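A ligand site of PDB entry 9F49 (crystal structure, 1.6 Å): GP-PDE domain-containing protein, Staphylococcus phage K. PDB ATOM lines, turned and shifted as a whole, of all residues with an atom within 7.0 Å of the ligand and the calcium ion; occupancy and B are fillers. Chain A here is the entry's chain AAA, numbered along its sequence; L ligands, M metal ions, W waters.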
ATOM      1  N   HIS A   8      14.463 -25.807 -18.340  1.00  0.00           N
ATOM      2  CA  HIS A   8      14.170 -25.528 -19.771  1.00  0.00           C
ATOM      3  C   HIS A   8      14.040 -26.854 -20.517  1.00  0.00           C
ATOM      4  O   HIS A   8      15.032 -27.566 -20.638  1.00  0.00           O
ATOM      5  CB  HIS A   8      15.278 -24.647 -20.355  1.00  0.00           C
ATOM      6  CG  HIS A   8      15.044 -24.210 -21.761  1.00  0.00           C
ATOM      7  ND1 HIS A   8      15.890 -24.599 -22.777  1.00  0.00           N
ATOM      8  CD2 HIS A   8      14.106 -23.419 -22.322  1.00  0.00           C
ATOM      9  CE1 HIS A   8      15.481 -24.053 -23.915  1.00  0.00           C
ATOM     10  NE2 HIS A   8      14.386 -23.324 -23.657  1.00  0.00           N
ATOM     11  N   ARG A   9      12.833 -27.139 -21.026  1.00  0.00           N
ATOM     12  CA  ARG A   9      12.463 -28.400 -21.708  1.00  0.00           C
ATOM     13  C   ARG A   9      12.852 -29.603 -20.840  1.00  0.00           C
ATOM     14  O   ARG A   9      13.118 -30.678 -21.402  1.00  0.00           O
ATOM     15  CB  ARG A   9      13.106 -28.455 -23.096  1.00  0.00           C
ATOM     16  CG  ARG A   9      13.008 -27.155 -23.876  1.00  0.00           C
ATOM     17  CD  ARG A   9      13.485 -27.229 -25.311  1.00  0.00           C
ATOM     18  NE  ARG A   9      13.630 -25.902 -25.879  1.00  0.00           N
ATOM     19  CZ  ARG A   9      14.315 -25.605 -26.987  1.00  0.00           C
ATOM     20  NH1 ARG A   9      14.905 -26.556 -27.687  1.00  0.00           N
ATOM     21  NH2 ARG A   9      14.431 -24.345 -27.366  1.00  0.00           N
ATOM     22  N   HIS A  18      12.279 -32.499 -23.469  1.00  0.00           N
ATOM     23  CA  HIS A  18      10.844 -32.882 -23.552  1.00  0.00           C
ATOM     24  C   HIS A  18      10.691 -34.393 -23.537  1.00  0.00           C
ATOM     25  O   HIS A  18      10.017 -34.940 -24.420  1.00  0.00           O
ATOM     26  CB  HIS A  18      10.184 -32.247 -24.777  1.00  0.00           C
ATOM     27  CG  HIS A  18      10.135 -30.768 -24.661  1.00  0.00           C
ATOM     28  ND1 HIS A  18       9.746 -30.145 -23.494  1.00  0.00           N
ATOM     29  CD2 HIS A  18      10.380 -29.797 -25.562  1.00  0.00           C
ATOM     30  CE1 HIS A  18       9.778 -28.840 -23.669  1.00  0.00           C
ATOM     31  NE2 HIS A  18      10.155 -28.603 -24.926  1.00  0.00           N
ATOM     32  N   GLU A  35       9.483 -27.196 -17.588  1.00  0.00           N
ATOM     33  CA  GLU A  35       8.992 -26.352 -18.704  1.00  0.00           C
ATOM     34  C   GLU A  35       8.605 -27.235 -19.894  1.00  0.00           C
ATOM     35  O   GLU A  35       9.462 -27.986 -20.388  1.00  0.00           O
ATOM     36  CB  GLU A  35      10.057 -25.334 -19.099  1.00  0.00           C
ATOM     37  CG  GLU A  35       9.499 -24.288 -20.044  1.00  0.00           C
ATOM     38  CD  GLU A  35      10.193 -24.117 -21.382  1.00  0.00           C
ATOM     39  OE1 GLU A  35      11.180 -24.818 -21.660  1.00  0.00           O
ATOM     40  OE2 GLU A  35       9.723 -23.239 -22.153  1.00  0.00           O
ATOM     41  N   LEU A  36       7.345 -27.148 -20.312  1.00  0.00           N
ATOM     42  CA  LEU A  36       6.788 -27.851 -21.491  1.00  0.00           C
ATOM     43  C   LEU A  36       6.607 -26.817 -22.611  1.00  0.00           C
ATOM     44  O   LEU A  36       6.099 -25.719 -22.314  1.00  0.00           O
ATOM     45  CB  LEU A  36       5.435 -28.472 -21.142  1.00  0.00           C
ATOM     46  CG  LEU A  36       5.447 -29.741 -20.294  1.00  0.00           C
ATOM     47  CD1 LEU A  36       6.168 -29.541 -18.980  1.00  0.00           C
ATOM     48  CD2 LEU A  36       4.018 -30.224 -20.062  1.00  0.00           C
ATOM     49  N   ASP A  37       6.987 -27.174 -23.837  1.00  0.00           N
ATOM     50  CA  ASP A  37       6.542 -26.500 -25.085  1.00  0.00           C
ATOM     51  C   ASP A  37       5.518 -27.441 -25.708  1.00  0.00           C
ATOM     52  O   ASP A  37       5.792 -28.646 -25.727  1.00  0.00           O
ATOM     53  CB  ASP A  37       7.682 -26.284 -26.073  1.00  0.00           C
ATOM     54  CG  ASP A  37       8.822 -25.421 -25.550  1.00  0.00           C
ATOM     55  OD1 ASP A  37       8.551 -24.316 -25.076  1.00  0.00           O
ATOM     56  OD2 ASP A  37       9.981 -25.890 -25.619  1.00  0.00           O
ATOM     57  N   HIS A  50       9.286 -28.714 -28.994  1.00  0.00           N
ATOM     58  CA  HIS A  50       9.650 -27.287 -29.186  1.00  0.00           C
ATOM     59  C   HIS A  50       9.338 -26.861 -30.626  1.00  0.00           C
ATOM     60  O   HIS A  50       8.595 -25.861 -30.815  1.00  0.00           O
ATOM     61  CB  HIS A  50      11.108 -27.048 -28.825  1.00  0.00           C
ATOM     62  CG  HIS A  50      11.505 -25.665 -29.181  1.00  0.00           C
ATOM     63  ND1 HIS A  50      11.999 -25.346 -30.432  1.00  0.00           N
ATOM     64  CD2 HIS A  50      11.400 -24.516 -28.497  1.00  0.00           C
ATOM     65  CE1 HIS A  50      12.222 -24.047 -30.482  1.00  0.00           C
ATOM     66  NE2 HIS A  50      11.868 -23.512 -29.308  1.00  0.00           N
ATOM     67  N   TYR A 101       5.442 -25.058 -16.107  1.00  0.00           N
ATOM     68  CA  TYR A 101       5.612 -23.783 -16.847  1.00  0.00           C
ATOM     69  C   TYR A 101       5.408 -24.133 -18.323  1.00  0.00           C
ATOM     70  O   TYR A 101       6.266 -24.800 -18.906  1.00  0.00           O
ATOM     71  CB  TYR A 101       6.979 -23.172 -16.506  1.00  0.00           C
ATOM     72  CG  TYR A 101       7.046 -21.667 -16.589  1.00  0.00           C
ATOM     73  CD1 TYR A 101       6.860 -21.020 -17.786  1.00  0.00           C
ATOM     74  CD2 TYR A 101       7.331 -20.894 -15.481  1.00  0.00           C
ATOM     75  CE1 TYR A 101       6.935 -19.649 -17.899  1.00  0.00           C
ATOM     76  CE2 TYR A 101       7.404 -19.511 -15.566  1.00  0.00           C
ATOM     77  CZ  TYR A 101       7.196 -18.873 -16.783  1.00  0.00           C
ATOM     78  OH  TYR A 101       7.285 -17.509 -16.903  1.00  0.00           O
ATOM     79  N   GLU A 103       4.301 -23.564 -22.345  1.00  0.00           N
ATOM     80  CA  GLU A 103       4.236 -22.659 -23.511  1.00  0.00           C
ATOM     81  C   GLU A 103       3.284 -23.202 -24.578  1.00  0.00           C
ATOM     82  O   GLU A 103       3.439 -24.359 -25.017  1.00  0.00           O
ATOM     83  CB  GLU A 103       5.624 -22.439 -24.103  1.00  0.00           C
ATOM     84  CG  GLU A 103       5.619 -21.418 -25.227  1.00  0.00           C
ATOM     85  CD  GLU A 103       6.999 -21.025 -25.729  1.00  0.00           C
ATOM     86  OE1 GLU A 103       7.996 -21.418 -25.080  1.00  0.00           O
ATOM     87  OE2 GLU A 103       7.077 -20.344 -26.780  1.00  0.00           O
ATOM     88  N   LYS A 105       2.928 -22.950 -28.284  1.00  0.00           N
ATOM     89  CA  LYS A 105       3.777 -22.567 -29.439  1.00  0.00           C
ATOM     90  C   LYS A 105       2.885 -21.991 -30.525  1.00  0.00           C
ATOM     91  O   LYS A 105       1.674 -22.263 -30.540  1.00  0.00           O
ATOM     92  CB  LYS A 105       4.608 -23.770 -29.908  1.00  0.00           C
ATOM     93  CG  LYS A 105       5.845 -24.042 -29.055  1.00  0.00           C
ATOM     94  CD  LYS A 105       6.841 -22.888 -29.121  1.00  0.00           C
ATOM     95  CE  LYS A 105       8.105 -23.096 -28.324  1.00  0.00           C
ATOM     96  NZ  LYS A 105       8.913 -21.854 -28.288  1.00  0.00           N
ATOM     97  N   GLN A 138       2.799 -19.580 -20.578  1.00  0.00           N
ATOM     98  CA  GLN A 138       3.657 -18.601 -21.287  1.00  0.00           C
ATOM     99  C   GLN A 138       3.395 -18.711 -22.791  1.00  0.00           C
ATOM    100  O   GLN A 138       3.024 -19.801 -23.262  1.00  0.00           O
ATOM    101  CB  GLN A 138       5.145 -18.838 -20.995  1.00  0.00           C
ATOM    102  CG  GLN A 138       5.535 -20.301 -21.126  1.00  0.00           C
ATOM    103  CD  GLN A 138       7.014 -20.600 -21.201  1.00  0.00           C
ATOM    104  OE1 GLN A 138       7.850 -19.721 -21.314  1.00  0.00           O
ATOM    105  NE2 GLN A 138       7.339 -21.889 -21.170  1.00  0.00           N
ATOM    106  N   SER A 139       3.558 -17.617 -23.510  1.00  0.00           N
ATOM    107  CA  SER A 139       3.479 -17.633 -24.986  1.00  0.00           C
ATOM    108  C   SER A 139       4.121 -16.377 -25.576  1.00  0.00           C
ATOM    109  O   SER A 139       4.147 -15.332 -24.904  1.00  0.00           O
ATOM    110  CB  SER A 139       2.055 -17.766 -25.433  1.00  0.00           C
ATOM    111  OG  SER A 139       1.980 -18.095 -26.811  1.00  0.00           O
ATOM    112  N   PHE A 140       4.647 -16.506 -26.789  1.00  0.00           N
ATOM    113  CA  PHE A 140       4.974 -15.360 -27.681  1.00  0.00           C
ATOM    114  C   PHE A 140       3.687 -14.817 -28.314  1.00  0.00           C
ATOM    115  O   PHE A 140       3.701 -13.669 -28.784  1.00  0.00           O
ATOM    116  CB  PHE A 140       5.942 -15.791 -28.779  1.00  0.00           C
ATOM    117  CG  PHE A 140       7.382 -15.935 -28.335  1.00  0.00           C
ATOM    118  CD1 PHE A 140       7.862 -17.149 -27.901  1.00  0.00           C
ATOM    119  CD2 PHE A 140       8.251 -14.856 -28.378  1.00  0.00           C
ATOM    120  CE1 PHE A 140       9.189 -17.288 -27.520  1.00  0.00           C
ATOM    121  CE2 PHE A 140       9.568 -14.992 -27.978  1.00  0.00           C
ATOM    122  CZ  PHE A 140      10.049 -16.214 -27.562  1.00  0.00           C
ATOM    123  N   LEU A 160       6.209 -13.925 -23.436  1.00  0.00           N
ATOM    124  CA  LEU A 160       7.574 -14.207 -23.927  1.00  0.00           C
ATOM    125  C   LEU A 160       7.964 -13.129 -24.939  1.00  0.00           C
ATOM    126  O   LEU A 160       7.141 -12.816 -25.845  1.00  0.00           O
ATOM    127  CB  LEU A 160       7.629 -15.601 -24.567  1.00  0.00           C
ATOM    128  CG  LEU A 160       7.611 -16.748 -23.577  1.00  0.00           C
ATOM    129  CD1 LEU A 160       7.243 -18.054 -24.251  1.00  0.00           C
ATOM    130  CD2 LEU A 160       8.965 -16.869 -22.866  1.00  0.00           C
ATOM    131  N   ALA A 181       8.697 -12.298 -19.726  1.00  0.00           N
ATOM    132  CA  ALA A 181       9.734 -13.335 -19.827  1.00  0.00           C
ATOM    133  C   ALA A 181      10.634 -12.966 -20.994  1.00  0.00           C
ATOM    134  O   ALA A 181      10.398 -13.398 -22.122  1.00  0.00           O
ATOM    135  CB  ALA A 181       9.089 -14.682 -19.971  1.00  0.00           C
ATOM    136  N   HIS A 203      11.039 -13.185 -15.734  1.00  0.00           N
ATOM    137  CA  HIS A 203      11.578 -14.564 -15.868  1.00  0.00           C
ATOM    138  C   HIS A 203      12.456 -14.615 -17.110  1.00  0.00           C
ATOM    139  O   HIS A 203      11.916 -14.579 -18.217  1.00  0.00           O
ATOM    140  CB  HIS A 203      10.435 -15.579 -15.936  1.00  0.00           C
ATOM    141  CG  HIS A 203       9.562 -15.596 -14.741  1.00  0.00           C
ATOM    142  ND1 HIS A 203       8.297 -16.140 -14.765  1.00  0.00           N
ATOM    143  CD2 HIS A 203       9.764 -15.169 -13.471  1.00  0.00           C
ATOM    144  CE1 HIS A 203       7.742 -16.027 -13.580  1.00  0.00           C
ATOM    145  NE2 HIS A 203       8.631 -15.432 -12.756  1.00  0.00           N
ATOM    146  N   ALA A 204      13.763 -14.682 -16.924  1.00  0.00           N
ATOM    147  CA  ALA A 204      14.764 -14.551 -18.006  1.00  0.00           C
ATOM    148  C   ALA A 204      15.068 -15.918 -18.629  1.00  0.00           C
ATOM    149  O   ALA A 204      15.145 -16.903 -17.895  1.00  0.00           O
ATOM    150  CB  ALA A 204      16.016 -13.938 -17.436  1.00  0.00           C
ATOM    151  N   TRP A 205      15.264 -15.966 -19.953  1.00  0.00           N
ATOM    152  CA  TRP A 205      15.596 -17.218 -20.687  1.00  0.00           C
ATOM    153  C   TRP A 205      16.642 -16.930 -21.755  1.00  0.00           C
ATOM    154  O   TRP A 205      16.699 -15.813 -22.263  1.00  0.00           O
ATOM    155  CB  TRP A 205      14.337 -17.780 -21.355  1.00  0.00           C
ATOM    156  CG  TRP A 205      13.675 -16.817 -22.294  1.00  0.00           C
ATOM    157  CD1 TRP A 205      12.674 -15.929 -21.998  1.00  0.00           C
ATOM    158  CD2 TRP A 205      13.925 -16.661 -23.700  1.00  0.00           C
ATOM    159  NE1 TRP A 205      12.316 -15.230 -23.110  1.00  0.00           N
ATOM    160  CE2 TRP A 205      13.057 -15.652 -24.174  1.00  0.00           C
ATOM    161  CE3 TRP A 205      14.802 -17.279 -24.607  1.00  0.00           C
ATOM    162  CZ2 TRP A 205      13.046 -15.251 -25.505  1.00  0.00           C
ATOM    163  CZ3 TRP A 205      14.793 -16.858 -25.925  1.00  0.00           C
ATOM    164  CH2 TRP A 205      13.924 -15.859 -26.362  1.00  0.00           C
ATOM    165  N   THR A 206      17.443 -17.927 -22.172  1.00  0.00           N
ATOM    166  CA  THR A 206      17.735 -19.159 -21.461  1.00  0.00           C
ATOM    167  C   THR A 206      19.200 -19.061 -21.007  1.00  0.00           C
ATOM    168  O   THR A 206      20.075 -18.982 -21.880  1.00  0.00           O
ATOM    169  CB  THR A 206      17.513 -20.393 -22.350  1.00  0.00           C
ATOM    170  OG1 THR A 206      16.126 -20.457 -22.693  1.00  0.00           O
ATOM    171  CG2 THR A 206      17.940 -21.683 -21.692  1.00  0.00           C
ATOM    172  N   PHE A 225      15.058 -19.564 -16.786  1.00  0.00           N
ATOM    173  CA  PHE A 225      15.062 -20.869 -17.467  1.00  0.00           C
ATOM    174  C   PHE A 225      16.511 -21.221 -17.782  1.00  0.00           C
ATOM    175  O   PHE A 225      17.242 -20.355 -18.278  1.00  0.00           O
ATOM    176  CB  PHE A 225      14.280 -20.794 -18.781  1.00  0.00           C
ATOM    177  CG  PHE A 225      12.857 -20.321 -18.721  1.00  0.00           C
ATOM    178  CD1 PHE A 225      12.562 -18.978 -18.512  1.00  0.00           C
ATOM    179  CD2 PHE A 225      11.817 -21.184 -19.020  1.00  0.00           C
ATOM    180  CE1 PHE A 225      11.247 -18.535 -18.518  1.00  0.00           C
ATOM    181  CE2 PHE A 225      10.498 -20.733 -19.030  1.00  0.00           C
ATOM    182  CZ  PHE A 225      10.228 -19.406 -18.780  1.00  0.00           C
HETATM  183  O1  LIG L   1       9.896 -20.260 -22.867  1.00  0.00           O
HETATM  184  C1  LIG L   1      11.149 -19.661 -22.574  1.00  0.00           C
HETATM  185  C2  LIG L   1      12.091 -19.961 -23.707  1.00  0.00           C
HETATM  186  O2  LIG L   1      12.170 -21.386 -23.821  1.00  0.00           O
HETATM  187  C3  LIG L   1      11.598 -19.363 -25.003  1.00  0.00           C
HETATM  188  O3  LIG L   1      12.388 -19.781 -26.120  1.00  0.00           O
HETATM  189  O4  LIG L   1      12.544 -21.106 -28.171  1.00  0.00           O
HETATM  190  O5  LIG L   1      13.449 -22.072 -26.029  1.00  0.00           O
HETATM  191  O6  LIG L   1      10.921 -21.878 -26.376  1.00  0.00           O
HETATM  192  P1  LIG L   1      12.314 -21.301 -26.683  1.00  0.00           P
HETATM  193 CA    CA M   1       9.928 -22.426 -24.293  1.00  0.00          CA
HETATM  194  O   HOH W   1      15.107 -21.613 -29.169  1.00  0.00           O
HETATM  195  O   HOH W   2      11.525 -24.246 -24.309  1.00  0.00           O
HETATM  196  O   HOH W   3      15.842 -20.904 -25.470  1.00  0.00           O
HETATM  197  O   HOH W   4      12.280 -18.847 -29.604  1.00  0.00           O
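Of the 20 residues printed, 3 come within 4 Å of the calcium ion.
The calcium ion is bound by OE2 of Glu 35 (2.3 Å), OE1 of Glu 103 (2.3 Å), O6 of the ligand (2.4 Å), water W2 (2.4 Å), OD1 of Asp 37 (2.5 Å), O2 of the ligand (2.5 Å) and O1 of the ligand (2.6 Å). The calcium ion has seven donor atoms within binding distance.
Water W2 lies within hydrogen-bond range of OD2 of Asp 37 (2.6 Å), OE1 of Glu 35 (2.7 Å), NE2 of His 8 (3.1 Å), NE of Arg 9 (3.1 Å) and O5 of the ligand (3.4 Å). Water W3 lies within hydrogen-bond range of an oxygen (O5) of the ligand, the side-chain hydroxyl of Thr 206 and a ring nitrogen (NE2) of His 8. Water W1 bridges an oxygen (O4) of the ligand and the guanidinium group of Arg 9.
CD2 of Leu 160 touches O1 of the ligand, 3.5 Å away. Trp 205 touches the ligand (CD2 to C2, 3.8 Å). CE2 of Phe 225 touches C1 of the ligand (3.8 Å). Within 4 Å of the ligand: His 8, Arg 9, Glu 35, Asp 37, His 50, Glu 103, Lys 105, Gln 138, Leu 160, Trp 205 and Phe 225.
OE1 of Gln 138 sits close to O1 of the ligand, 2.6 Å away. An oxygen (O4) of the ligand sits at hydrogen-bond distance from a ring nitrogen (NE2) of His 50. O4 of the ligand is in salt-bridge range of NZ of Lys 105 (3.7 Å). The guanidinium group of Arg 9 lies within salt-bridge range of an oxygen (O5) of the ligand (2.8 Å). An oxygen (O5) of the ligand lies within hydrogen-bond range of a ring nitrogen (NE2) of His 8 (2.8 Å).
NE2 of Gln 138 sits close to OE2 of Glu 35. OE1 of Glu 35 is in hydrogen-bond range of N of Arg 9 (2.9 Å). N of Glu 103 lies within hydrogen-bond range of O of Leu 36, 2.8 Å away. The side-chain carboxylate (OD2) of Asp 37 is in salt-bridge range of the guanidinium group (NE) of Arg 9, at 3.7 Å. NH2 of Arg 9 lies close to NE2 of His 50 (3.3 Å). A ring nitrogen (NE2) of His 8 lies close to the guanidinium group (NE) of Arg 9 (3.5 Å). N of His 18 sits at hydrogen-bond distance from O of Arg 9, 2.9 Å away. The backbone NH (N) of Phe 225 is in hydrogen-bond range of the backbone carbonyl oxygen (O) of Ala 204 (2.9 Å).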
